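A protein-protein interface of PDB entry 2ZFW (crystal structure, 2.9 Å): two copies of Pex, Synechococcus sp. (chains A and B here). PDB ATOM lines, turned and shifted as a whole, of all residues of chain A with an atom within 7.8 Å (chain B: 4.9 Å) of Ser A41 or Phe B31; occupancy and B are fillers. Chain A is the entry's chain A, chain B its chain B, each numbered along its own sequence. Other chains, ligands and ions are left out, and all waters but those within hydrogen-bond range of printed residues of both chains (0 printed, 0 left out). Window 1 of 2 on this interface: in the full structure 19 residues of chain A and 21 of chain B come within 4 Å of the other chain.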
ATOM      1  N   HIS A  38     -13.770   5.619 -24.172  1.00  0.00           N
ATOM      2  CA  HIS A  38     -14.018   4.501 -23.284  1.00  0.00           C
ATOM      3  C   HIS A  38     -12.825   3.556 -23.307  1.00  0.00           C
ATOM      4  O   HIS A  38     -12.490   2.993 -24.356  1.00  0.00           O
ATOM      5  CB  HIS A  38     -15.262   3.744 -23.725  1.00  0.00           C
ATOM      6  CG  HIS A  38     -16.464   4.010 -22.873  1.00  0.00           C
ATOM      7  ND1 HIS A  38     -16.947   5.280 -22.646  1.00  0.00           N
ATOM      8  CD2 HIS A  38     -17.273   3.171 -22.185  1.00  0.00           C
ATOM      9  CE1 HIS A  38     -18.002   5.213 -21.855  1.00  0.00           C
ATOM     10  NE2 HIS A  38     -18.220   3.944 -21.560  1.00  0.00           N
ATOM     11  N   TYR A  39     -12.168   3.394 -22.160  1.00  0.00           N
ATOM     12  CA  TYR A  39     -11.023   2.489 -22.071  1.00  0.00           C
ATOM     13  C   TYR A  39     -11.548   1.052 -22.091  1.00  0.00           C
ATOM     14  O   TYR A  39     -12.402   0.687 -21.281  1.00  0.00           O
ATOM     15  CB  TYR A  39     -10.241   2.738 -20.788  1.00  0.00           C
ATOM     16  CG  TYR A  39      -9.375   3.971 -20.823  1.00  0.00           C
ATOM     17  CD1 TYR A  39      -9.938   5.237 -20.795  1.00  0.00           C
ATOM     18  CD2 TYR A  39      -7.996   3.871 -20.920  1.00  0.00           C
ATOM     19  CE1 TYR A  39      -9.144   6.385 -20.868  1.00  0.00           C
ATOM     20  CE2 TYR A  39      -7.195   5.000 -20.995  1.00  0.00           C
ATOM     21  CZ  TYR A  39      -7.772   6.260 -20.972  1.00  0.00           C
ATOM     22  OH  TYR A  39      -6.997   7.397 -21.097  1.00  0.00           O
ATOM     23  N   LEU A  40     -11.055   0.241 -23.023  1.00  0.00           N
ATOM     24  CA  LEU A  40     -11.526  -1.138 -23.133  1.00  0.00           C
ATOM     25  C   LEU A  40     -11.370  -1.902 -21.824  1.00  0.00           C
ATOM     26  O   LEU A  40     -10.439  -1.657 -21.051  1.00  0.00           O
ATOM     27  CB  LEU A  40     -10.755  -1.892 -24.221  1.00  0.00           C
ATOM     28  CG  LEU A  40     -10.433  -1.242 -25.575  1.00  0.00           C
ATOM     29  CD1 LEU A  40      -9.996  -2.341 -26.530  1.00  0.00           C
ATOM     30  CD2 LEU A  40     -11.636  -0.515 -26.151  1.00  0.00           C
ATOM     31  N   SER A  41     -12.294  -2.826 -21.587  1.00  0.00           N
ATOM     32  CA  SER A  41     -12.246  -3.676 -20.408  1.00  0.00           C
ATOM     33  C   SER A  41     -11.300  -4.802 -20.809  1.00  0.00           C
ATOM     34  O   SER A  41     -10.866  -4.863 -21.967  1.00  0.00           O
ATOM     35  CB  SER A  41     -13.626  -4.246 -20.100  1.00  0.00           C
ATOM     36  OG  SER A  41     -14.118  -5.033 -21.169  1.00  0.00           O
ATOM     37  N   LYS A  42     -10.961  -5.686 -19.874  1.00  0.00           N
ATOM     38  CA  LYS A  42     -10.050  -6.787 -20.204  1.00  0.00           C
ATOM     39  C   LYS A  42     -10.666  -7.584 -21.351  1.00  0.00           C
ATOM     40  O   LYS A  42      -9.969  -7.985 -22.286  1.00  0.00           O
ATOM     41  CB  LYS A  42      -9.841  -7.701 -18.993  1.00  0.00           C
ATOM     42  CG  LYS A  42     -10.195  -7.033 -17.678  1.00  0.00           C
ATOM     43  CD  LYS A  42     -11.720  -7.023 -17.446  1.00  0.00           C
ATOM     44  CE  LYS A  42     -12.168  -6.029 -16.375  1.00  0.00           C
ATOM     45  NZ  LYS A  42     -13.660  -6.009 -16.325  1.00  0.00           N
ATOM     46  N   GLU A  43     -11.979  -7.799 -21.270  1.00  0.00           N
ATOM     47  CA  GLU A  43     -12.708  -8.540 -22.286  1.00  0.00           C
ATOM     48  C   GLU A  43     -12.671  -7.860 -23.644  1.00  0.00           C
ATOM     49  O   GLU A  43     -12.448  -8.501 -24.663  1.00  0.00           O
ATOM     50  CB  GLU A  43     -14.157  -8.736 -21.862  1.00  0.00           C
ATOM     51  CG  GLU A  43     -14.316  -9.674 -20.682  1.00  0.00           C
ATOM     52  CD  GLU A  43     -14.024  -9.013 -19.347  1.00  0.00           C
ATOM     53  OE1 GLU A  43     -13.641  -7.830 -19.339  1.00  0.00           O
ATOM     54  OE2 GLU A  43     -14.189  -9.676 -18.304  1.00  0.00           O
ATOM     55  N   LEU A  44     -12.908  -6.557 -23.670  1.00  0.00           N
ATOM     56  CA  LEU A  44     -12.868  -5.839 -24.937  1.00  0.00           C
ATOM     57  C   LEU A  44     -11.490  -5.997 -25.578  1.00  0.00           C
ATOM     58  O   LEU A  44     -11.364  -6.095 -26.795  1.00  0.00           O
ATOM     59  CB  LEU A  44     -13.196  -4.360 -24.722  1.00  0.00           C
ATOM     60  CG  LEU A  44     -14.681  -4.140 -24.492  1.00  0.00           C
ATOM     61  CD1 LEU A  44     -14.952  -2.758 -23.949  1.00  0.00           C
ATOM     62  CD2 LEU A  44     -15.388  -4.362 -25.798  1.00  0.00           C
ATOM     63  N   ALA A  45     -10.459  -6.042 -24.742  1.00  0.00           N
ATOM     64  CA  ALA A  45      -9.083  -6.195 -25.211  1.00  0.00           C
ATOM     65  C   ALA A  45      -8.836  -7.545 -25.893  1.00  0.00           C
ATOM     66  O   ALA A  45      -8.373  -7.600 -27.036  1.00  0.00           O
ATOM     67  CB  ALA A  45      -8.110  -6.016 -24.037  1.00  0.00           C
ATOM     68  N   VAL A  46      -9.140  -8.626 -25.182  1.00  0.00           N
ATOM     69  CA  VAL A  46      -8.943  -9.965 -25.705  1.00  0.00           C
ATOM     70  C   VAL A  46      -9.586 -10.123 -27.065  1.00  0.00           C
ATOM     71  O   VAL A  46      -9.008 -10.754 -27.953  1.00  0.00           O
ATOM     72  CB  VAL A  46      -9.509 -11.037 -24.747  1.00  0.00           C
ATOM     73  CG1 VAL A  46      -9.401 -12.420 -25.379  1.00  0.00           C
ATOM     74  CG2 VAL A  46      -8.730 -11.026 -23.435  1.00  0.00           C
ATOM     75  N   CYS A  47     -10.771  -9.543 -27.237  1.00  0.00           N
ATOM     76  CA  CYS A  47     -11.479  -9.624 -28.513  1.00  0.00           C
ATOM     77  C   CYS A  47     -10.862  -8.677 -29.531  1.00  0.00           C
ATOM     78  O   CYS A  47     -10.501  -9.103 -30.629  1.00  0.00           O
ATOM     79  CB  CYS A  47     -12.957  -9.330 -28.294  1.00  0.00           C
ATOM     80  SG  CYS A  47     -13.699 -10.515 -27.122  1.00  0.00           S
ATOM     81  N   TYR A  48     -10.713  -7.406 -29.154  1.00  0.00           N
ATOM     82  CA  TYR A  48     -10.093  -6.410 -30.032  1.00  0.00           C
ATOM     83  C   TYR A  48      -8.752  -6.921 -30.559  1.00  0.00           C
ATOM     84  O   TYR A  48      -8.419  -6.696 -31.732  1.00  0.00           O
ATOM     85  CB  TYR A  48      -9.844  -5.082 -29.294  1.00  0.00           C
ATOM     86  CG  TYR A  48      -8.787  -4.210 -29.962  1.00  0.00           C
ATOM     87  CD1 TYR A  48      -9.062  -3.526 -31.139  1.00  0.00           C
ATOM     88  CD2 TYR A  48      -7.479  -4.163 -29.468  1.00  0.00           C
ATOM     89  CE1 TYR A  48      -8.072  -2.825 -31.816  1.00  0.00           C
ATOM     90  CE2 TYR A  48      -6.470  -3.469 -30.144  1.00  0.00           C
ATOM     91  CZ  TYR A  48      -6.779  -2.802 -31.317  1.00  0.00           C
ATOM     92  OH  TYR A  48      -5.795  -2.110 -31.986  1.00  0.00           O
ATOM     93  N   TYR A  74     -12.179   5.203 -28.100  1.00  0.00           N
ATOM     94  CA  TYR A  74     -11.611   4.173 -27.266  1.00  0.00           C
ATOM     95  C   TYR A  74     -10.134   4.357 -27.012  1.00  0.00           C
ATOM     96  O   TYR A  74      -9.445   5.059 -27.742  1.00  0.00           O
ATOM     97  CB  TYR A  74     -11.841   2.826 -27.925  1.00  0.00           C
ATOM     98  CG  TYR A  74     -13.297   2.482 -28.081  1.00  0.00           C
ATOM     99  CD1 TYR A  74     -14.040   2.011 -26.996  1.00  0.00           C
ATOM    100  CD2 TYR A  74     -13.940   2.638 -29.308  1.00  0.00           C
ATOM    101  CE1 TYR A  74     -15.383   1.701 -27.127  1.00  0.00           C
ATOM    102  CE2 TYR A  74     -15.288   2.331 -29.449  1.00  0.00           C
ATOM    103  CZ  TYR A  74     -15.998   1.861 -28.348  1.00  0.00           C
ATOM    104  OH  TYR A  74     -17.322   1.531 -28.467  1.00  0.00           O
ATOM    105  N   ARG A  75      -9.667   3.712 -25.951  1.00  0.00           N
ATOM    106  CA  ARG A  75      -8.265   3.716 -25.549  1.00  0.00           C
ATOM    107  C   ARG A  75      -7.979   2.338 -24.932  1.00  0.00           C
ATOM    108  O   ARG A  75      -8.906   1.605 -24.537  1.00  0.00           O
ATOM    109  CB  ARG A  75      -8.006   4.802 -24.509  1.00  0.00           C
ATOM    110  CG  ARG A  75      -8.030   6.201 -25.047  1.00  0.00           C
ATOM    111  CD  ARG A  75      -6.901   6.448 -26.003  1.00  0.00           C
ATOM    112  NE  ARG A  75      -6.873   7.835 -26.450  1.00  0.00           N
ATOM    113  CZ  ARG A  75      -7.830   8.423 -27.164  1.00  0.00           C
ATOM    114  NH1 ARG A  75      -8.914   7.751 -27.534  1.00  0.00           N
ATOM    115  NH2 ARG A  75      -7.705   9.700 -27.506  1.00  0.00           N
ATOM    116  N   LEU A  76      -6.698   1.991 -24.856  1.00  0.00           N
ATOM    117  CA  LEU A  76      -6.272   0.719 -24.274  1.00  0.00           C
ATOM    118  C   LEU A  76      -5.023   0.985 -23.449  1.00  0.00           C
ATOM    119  O   LEU A  76      -3.993   1.370 -23.977  1.00  0.00           O
ATOM    120  CB  LEU A  76      -5.941  -0.285 -25.378  1.00  0.00           C
ATOM    121  CG  LEU A  76      -5.690  -1.718 -24.936  1.00  0.00           C
ATOM    122  CD1 LEU A  76      -7.004  -2.375 -24.549  1.00  0.00           C
ATOM    123  CD2 LEU A  76      -5.028  -2.480 -26.045  1.00  0.00           C
ATOM    124  N   VAL A  80      -4.284  -3.777 -18.898  1.00  0.00           N
ATOM    125  CA  VAL A  80      -5.341  -4.526 -19.558  1.00  0.00           C
ATOM    126  C   VAL A  80      -4.826  -5.245 -20.815  1.00  0.00           C
ATOM    127  O   VAL A  80      -5.030  -6.445 -20.973  1.00  0.00           O
ATOM    128  CB  VAL A  80      -6.508  -3.585 -19.932  1.00  0.00           C
ATOM    129  CG1 VAL A  80      -7.671  -4.382 -20.459  1.00  0.00           C
ATOM    130  CG2 VAL A  80      -6.937  -2.787 -18.718  1.00  0.00           C
ATOM    131  N   LEU A  81      -4.151  -4.519 -21.704  1.00  0.00           N
ATOM    132  CA  LEU A  81      -3.627  -5.140 -22.910  1.00  0.00           C
ATOM    133  C   LEU A  81      -2.751  -6.327 -22.583  1.00  0.00           C
ATOM    134  O   LEU A  81      -2.711  -7.288 -23.350  1.00  0.00           O
ATOM    135  CB  LEU A  81      -2.823  -4.148 -23.752  1.00  0.00           C
ATOM    136  CG  LEU A  81      -1.914  -4.818 -24.803  1.00  0.00           C
ATOM    137  CD1 LEU A  81      -2.010  -4.121 -26.166  1.00  0.00           C
ATOM    138  CD2 LEU A  81      -0.497  -4.811 -24.292  1.00  0.00           C
ATOM    139  N   ALA A  84      -4.936  -9.349 -21.141  1.00  0.00           N
ATOM    140  CA  ALA A  84      -5.563  -9.924 -22.324  1.00  0.00           C
ATOM    141  C   ALA A  84      -4.557 -10.788 -23.074  1.00  0.00           C
ATOM    142  O   ALA A  84      -4.844 -11.933 -23.418  1.00  0.00           O
ATOM    143  CB  ALA A  84      -6.087  -8.813 -23.233  1.00  0.00           C
ATOM    144  N   TRP A 128     -16.069  -8.402 -31.119  1.00  0.00           N
ATOM    145  CA  TRP A 128     -15.561  -7.037 -31.114  1.00  0.00           C
ATOM    146  C   TRP A 128     -16.332  -6.313 -32.190  1.00  0.00           C
ATOM    147  O   TRP A 128     -17.012  -5.327 -31.917  1.00  0.00           O
ATOM    148  CB  TRP A 128     -14.053  -7.015 -31.420  1.00  0.00           C
ATOM    149  CG  TRP A 128     -13.454  -5.646 -31.629  1.00  0.00           C
ATOM    150  CD1 TRP A 128     -12.752  -5.230 -32.719  1.00  0.00           C
ATOM    151  CD2 TRP A 128     -13.488  -4.528 -30.726  1.00  0.00           C
ATOM    152  NE1 TRP A 128     -12.347  -3.921 -32.557  1.00  0.00           N
ATOM    153  CE2 TRP A 128     -12.785  -3.469 -31.341  1.00  0.00           C
ATOM    154  CE3 TRP A 128     -14.044  -4.316 -29.457  1.00  0.00           C
ATOM    155  CZ2 TRP A 128     -12.620  -2.228 -30.732  1.00  0.00           C
ATOM    156  CZ3 TRP A 128     -13.878  -3.084 -28.854  1.00  0.00           C
ATOM    157  CH2 TRP A 128     -13.173  -2.055 -29.492  1.00  0.00           C
ATOM    158  N   TYR A 131     -19.645  -5.259 -31.185  1.00  0.00           N
ATOM    159  CA  TYR A 131     -19.518  -4.147 -30.235  1.00  0.00           C
ATOM    160  C   TYR A 131     -19.275  -2.784 -30.894  1.00  0.00           C
ATOM    161  O   TYR A 131     -19.691  -1.746 -30.373  1.00  0.00           O
ATOM    162  CB  TYR A 131     -18.375  -4.428 -29.256  1.00  0.00           C
ATOM    163  CG  TYR A 131     -18.368  -3.528 -28.034  1.00  0.00           C
ATOM    164  CD1 TYR A 131     -19.157  -3.825 -26.924  1.00  0.00           C
ATOM    165  CD2 TYR A 131     -17.596  -2.370 -28.001  1.00  0.00           C
ATOM    166  CE1 TYR A 131     -19.181  -2.999 -25.817  1.00  0.00           C
ATOM    167  CE2 TYR A 131     -17.611  -1.536 -26.893  1.00  0.00           C
ATOM    168  CZ  TYR A 131     -18.408  -1.856 -25.803  1.00  0.00           C
ATOM    169  OH  TYR A 131     -18.436  -1.027 -24.700  1.00  0.00           O
ATOM    170  N   ASP B  27     -15.557 -15.742 -18.382  1.00  0.00           N
ATOM    171  CA  ASP B  27     -15.474 -14.322 -18.059  1.00  0.00           C
ATOM    172  C   ASP B  27     -15.801 -13.530 -19.327  1.00  0.00           C
ATOM    173  O   ASP B  27     -16.780 -12.790 -19.374  1.00  0.00           O
ATOM    174  CB  ASP B  27     -14.061 -13.969 -17.569  1.00  0.00           C
ATOM    175  CG  ASP B  27     -13.912 -14.070 -16.056  1.00  0.00           C
ATOM    176  OD1 ASP B  27     -14.350 -13.142 -15.345  1.00  0.00           O
ATOM    177  OD2 ASP B  27     -13.360 -15.080 -15.575  1.00  0.00           O
ATOM    178  N   ILE B  28     -14.982 -13.712 -20.357  1.00  0.00           N
ATOM    179  CA  ILE B  28     -15.167 -13.015 -21.616  1.00  0.00           C
ATOM    180  C   ILE B  28     -16.549 -13.235 -22.206  1.00  0.00           C
ATOM    181  O   ILE B  28     -17.031 -12.408 -22.976  1.00  0.00           O
ATOM    182  CB  ILE B  28     -14.125 -13.458 -22.648  1.00  0.00           C
ATOM    183  CG1 ILE B  28     -12.726 -13.367 -22.037  1.00  0.00           C
ATOM    184  CG2 ILE B  28     -14.210 -12.569 -23.885  1.00  0.00           C
ATOM    185  CD1 ILE B  28     -11.632 -13.971 -22.892  1.00  0.00           C
ATOM    186  N   TYR B  29     -17.190 -14.344 -21.857  1.00  0.00           N
ATOM    187  CA  TYR B  29     -18.524 -14.613 -22.384  1.00  0.00           C
ATOM    188  C   TYR B  29     -19.590 -14.136 -21.410  1.00  0.00           C
ATOM    189  O   TYR B  29     -20.784 -14.265 -21.673  1.00  0.00           O
ATOM    190  CB  TYR B  29     -18.696 -16.107 -22.680  1.00  0.00           C
ATOM    191  CG  TYR B  29     -19.316 -16.386 -24.044  1.00  0.00           C
ATOM    192  CD1 TYR B  29     -18.683 -15.964 -25.220  1.00  0.00           C
ATOM    193  CD2 TYR B  29     -20.551 -17.040 -24.157  1.00  0.00           C
ATOM    194  CE1 TYR B  29     -19.266 -16.181 -26.477  1.00  0.00           C
ATOM    195  CE2 TYR B  29     -21.141 -17.264 -25.407  1.00  0.00           C
ATOM    196  CZ  TYR B  29     -20.495 -16.832 -26.560  1.00  0.00           C
ATOM    197  OH  TYR B  29     -21.083 -17.044 -27.788  1.00  0.00           O
ATOM    198  N   ARG B  30     -19.145 -13.576 -20.289  1.00  0.00           N
ATOM    199  CA  ARG B  30     -20.049 -13.062 -19.264  1.00  0.00           C
ATOM    200  C   ARG B  30     -20.132 -11.540 -19.322  1.00  0.00           C
ATOM    201  O   ARG B  30     -21.162 -10.944 -18.984  1.00  0.00           O
ATOM    202  CB  ARG B  30     -19.581 -13.501 -17.871  1.00  0.00           C
ATOM    203  CG  ARG B  30     -20.369 -12.851 -16.736  1.00  0.00           C
ATOM    204  CD  ARG B  30     -20.108 -13.484 -15.374  1.00  0.00           C
ATOM    205  NE  ARG B  30     -18.690 -13.557 -15.026  1.00  0.00           N
ATOM    206  CZ  ARG B  30     -17.886 -14.565 -15.353  1.00  0.00           C
ATOM    207  NH1 ARG B  30     -18.357 -15.599 -16.041  1.00  0.00           N
ATOM    208  NH2 ARG B  30     -16.610 -14.544 -14.987  1.00  0.00           N
ATOM    209  N   PHE B  31     -19.035 -10.926 -19.760  1.00  0.00           N
ATOM    210  CA  PHE B  31     -18.937  -9.472 -19.882  1.00  0.00           C
ATOM    211  C   PHE B  31     -19.989  -8.926 -20.837  1.00  0.00           C
ATOM    212  O   PHE B  31     -20.611  -7.889 -20.570  1.00  0.00           O
ATOM    213  CB  PHE B  31     -17.555  -9.071 -20.401  1.00  0.00           C
ATOM    214  CG  PHE B  31     -17.439  -7.607 -20.745  1.00  0.00           C
ATOM    215  CD1 PHE B  31     -17.323  -6.648 -19.746  1.00  0.00           C
ATOM    216  CD2 PHE B  31     -17.457  -7.190 -22.070  1.00  0.00           C
ATOM    217  CE1 PHE B  31     -17.227  -5.304 -20.064  1.00  0.00           C
ATOM    218  CE2 PHE B  31     -17.361  -5.847 -22.391  1.00  0.00           C
ATOM    219  CZ  PHE B  31     -17.245  -4.904 -21.386  1.00  0.00           C
ATOM    220  N   PHE B  32     -20.172  -9.626 -21.954  1.00  0.00           N
ATOM    221  CA  PHE B  32     -21.140  -9.206 -22.947  1.00  0.00           C
ATOM    222  C   PHE B  32     -22.579  -9.388 -22.494  1.00  0.00           C
ATOM    223  O   PHE B  32     -23.451  -8.622 -22.892  1.00  0.00           O
ATOM    224  CB  PHE B  32     -20.922  -9.953 -24.253  1.00  0.00           C
ATOM    225  CG  PHE B  32     -19.696  -9.525 -25.001  1.00  0.00           C
ATOM    226  CD1 PHE B  32     -18.439  -9.666 -24.443  1.00  0.00           C
ATOM    227  CD2 PHE B  32     -19.797  -9.022 -26.288  1.00  0.00           C
ATOM    228  CE1 PHE B  32     -17.302  -9.318 -25.159  1.00  0.00           C
ATOM    229  CE2 PHE B  32     -18.666  -8.677 -27.000  1.00  0.00           C
ATOM    230  CZ  PHE B  32     -17.415  -8.827 -26.432  1.00  0.00           C
ATOM    231  N   GLN B  33     -22.836 -10.398 -21.667  1.00  0.00           N
ATOM    232  CA  GLN B  33     -24.193 -10.630 -21.179  1.00  0.00           C
ATOM    233  C   GLN B  33     -24.477  -9.650 -20.044  1.00  0.00           C
ATOM    234  O   GLN B  33     -25.493  -8.955 -20.049  1.00  0.00           O
ATOM    235  CB  GLN B  33     -24.344 -12.061 -20.663  1.00  0.00           C
ATOM    236  CG  GLN B  33     -23.589 -13.103 -21.477  1.00  0.00           C
ATOM    237  CD  GLN B  33     -24.036 -13.174 -22.925  1.00  0.00           C
ATOM    238  OE1 GLN B  33     -24.003 -12.175 -23.649  1.00  0.00           O
ATOM    239  NE2 GLN B  33     -24.448 -14.363 -23.360  1.00  0.00           N
ATOM    240  N   ASP B  34     -23.561  -9.584 -19.084  1.00  0.00           N
ATOM    241  CA  ASP B  34     -23.715  -8.693 -17.944  1.00  0.00           C
ATOM    242  C   ASP B  34     -22.653  -7.595 -17.984  1.00  0.00           C
ATOM    243  O   ASP B  34     -21.644  -7.663 -17.276  1.00  0.00           O
ATOM    244  CB  ASP B  34     -23.573  -9.483 -16.645  1.00  0.00           C
ATOM    245  CG  ASP B  34     -24.430  -8.933 -15.536  1.00  0.00           C
ATOM    246  OD1 ASP B  34     -24.515  -7.694 -15.408  1.00  0.00           O
ATOM    247  OD2 ASP B  34     -25.009  -9.746 -14.785  1.00  0.00           O
ATOM    248  N   PRO B  35     -22.853  -6.571 -18.818  1.00  0.00           N
ATOM    249  CA  PRO B  35     -21.836  -5.522 -18.851  1.00  0.00           C
ATOM    250  C   PRO B  35     -21.905  -4.636 -17.613  1.00  0.00           C
ATOM    251  O   PRO B  35     -22.988  -4.348 -17.107  1.00  0.00           O
ATOM    252  CB  PRO B  35     -22.176  -4.766 -20.127  1.00  0.00           C
ATOM    253  CG  PRO B  35     -23.671  -4.895 -20.189  1.00  0.00           C
ATOM    254  CD  PRO B  35     -23.898  -6.341 -19.830  1.00  0.00           C
ATOM    255  N   PRO B  36     -20.742  -4.206 -17.094  1.00  0.00           N
ATOM    256  CA  PRO B  36     -20.699  -3.344 -15.908  1.00  0.00           C
ATOM    257  C   PRO B  36     -21.479  -2.064 -16.187  1.00  0.00           C
ATOM    258  O   PRO B  36     -21.424  -1.524 -17.293  1.00  0.00           O
ATOM    259  CB  PRO B  36     -19.209  -3.072 -15.733  1.00  0.00           C
ATOM    260  CG  PRO B  36     -18.576  -4.314 -16.274  1.00  0.00           C
ATOM    261  CD  PRO B  36     -19.380  -4.558 -17.531  1.00  0.00           C
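The side-chain hydroxyl (OG) of Ser A41 lies within hydrogen-bond range of the side-chain carboxylate (OE1) of Glu A43 (3.4 Å). The side-chain hydroxyl (OG) of Ser A41 is in hydrogen-bond range of the backbone NH (N) of Leu A44, at 3.2 Å. NZ of Lys A42 is in salt-bridge range of OE1 of Glu A43 (3.5 Å). The side-chain sulfur (SG) of Cys A47 lies within hydrogen-bond range of the backbone carbonyl oxygen (O) of Glu A43 (3.4 Å).
CZ of Phe B31 touches OG of Ser A41 (3.1 Å). Glu A43 touches Ile B28 (CG to CA, 3.6 Å). Glu A43 touches Phe B31 (CG to CB, 3.3 Å). CG of Leu A44 touches CE2 of Phe B31, at 3.8 Å. Ile B28 touches Val A46 (CD1 to CG1, 3.7 Å). Ile B28 touches Cys A47.
Ser A41 touches just one residue of chain B: Phe B31. Lys A42 touches none of the printed residues of chain B. Of the printed residues of chain B, Val A46 touches Ile B28. Printed residues of chain A within 4 Å of Ile B28: Glu A43 (3.6 Å), Val A46 (3.7 Å) and Cys A47 (3.9 Å). Pro B36 touches none of the printed residues of chain A. The nearest residue of chain A that does not touch Phe B31 is Tyr A131 (4.8 Å).
Hydrophobic or aromatic side chains of chain A within 4 Å of the printed part of chain B: Leu A44 and Val A46. Along chain A the printed residues that touch a printed residue of chain B span positions 41 to 47. Hydrophobic or aromatic side chains of chain B within 4 Å of the printed part of chain A: Ile B28 and Phe B31. Among the printed residues, 6 pairs touch across the chains.
No position is printed for both chains. Of the 6 pairs that touch across the chains among the printed residues, none has its exchanged pair printed and touching as well.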
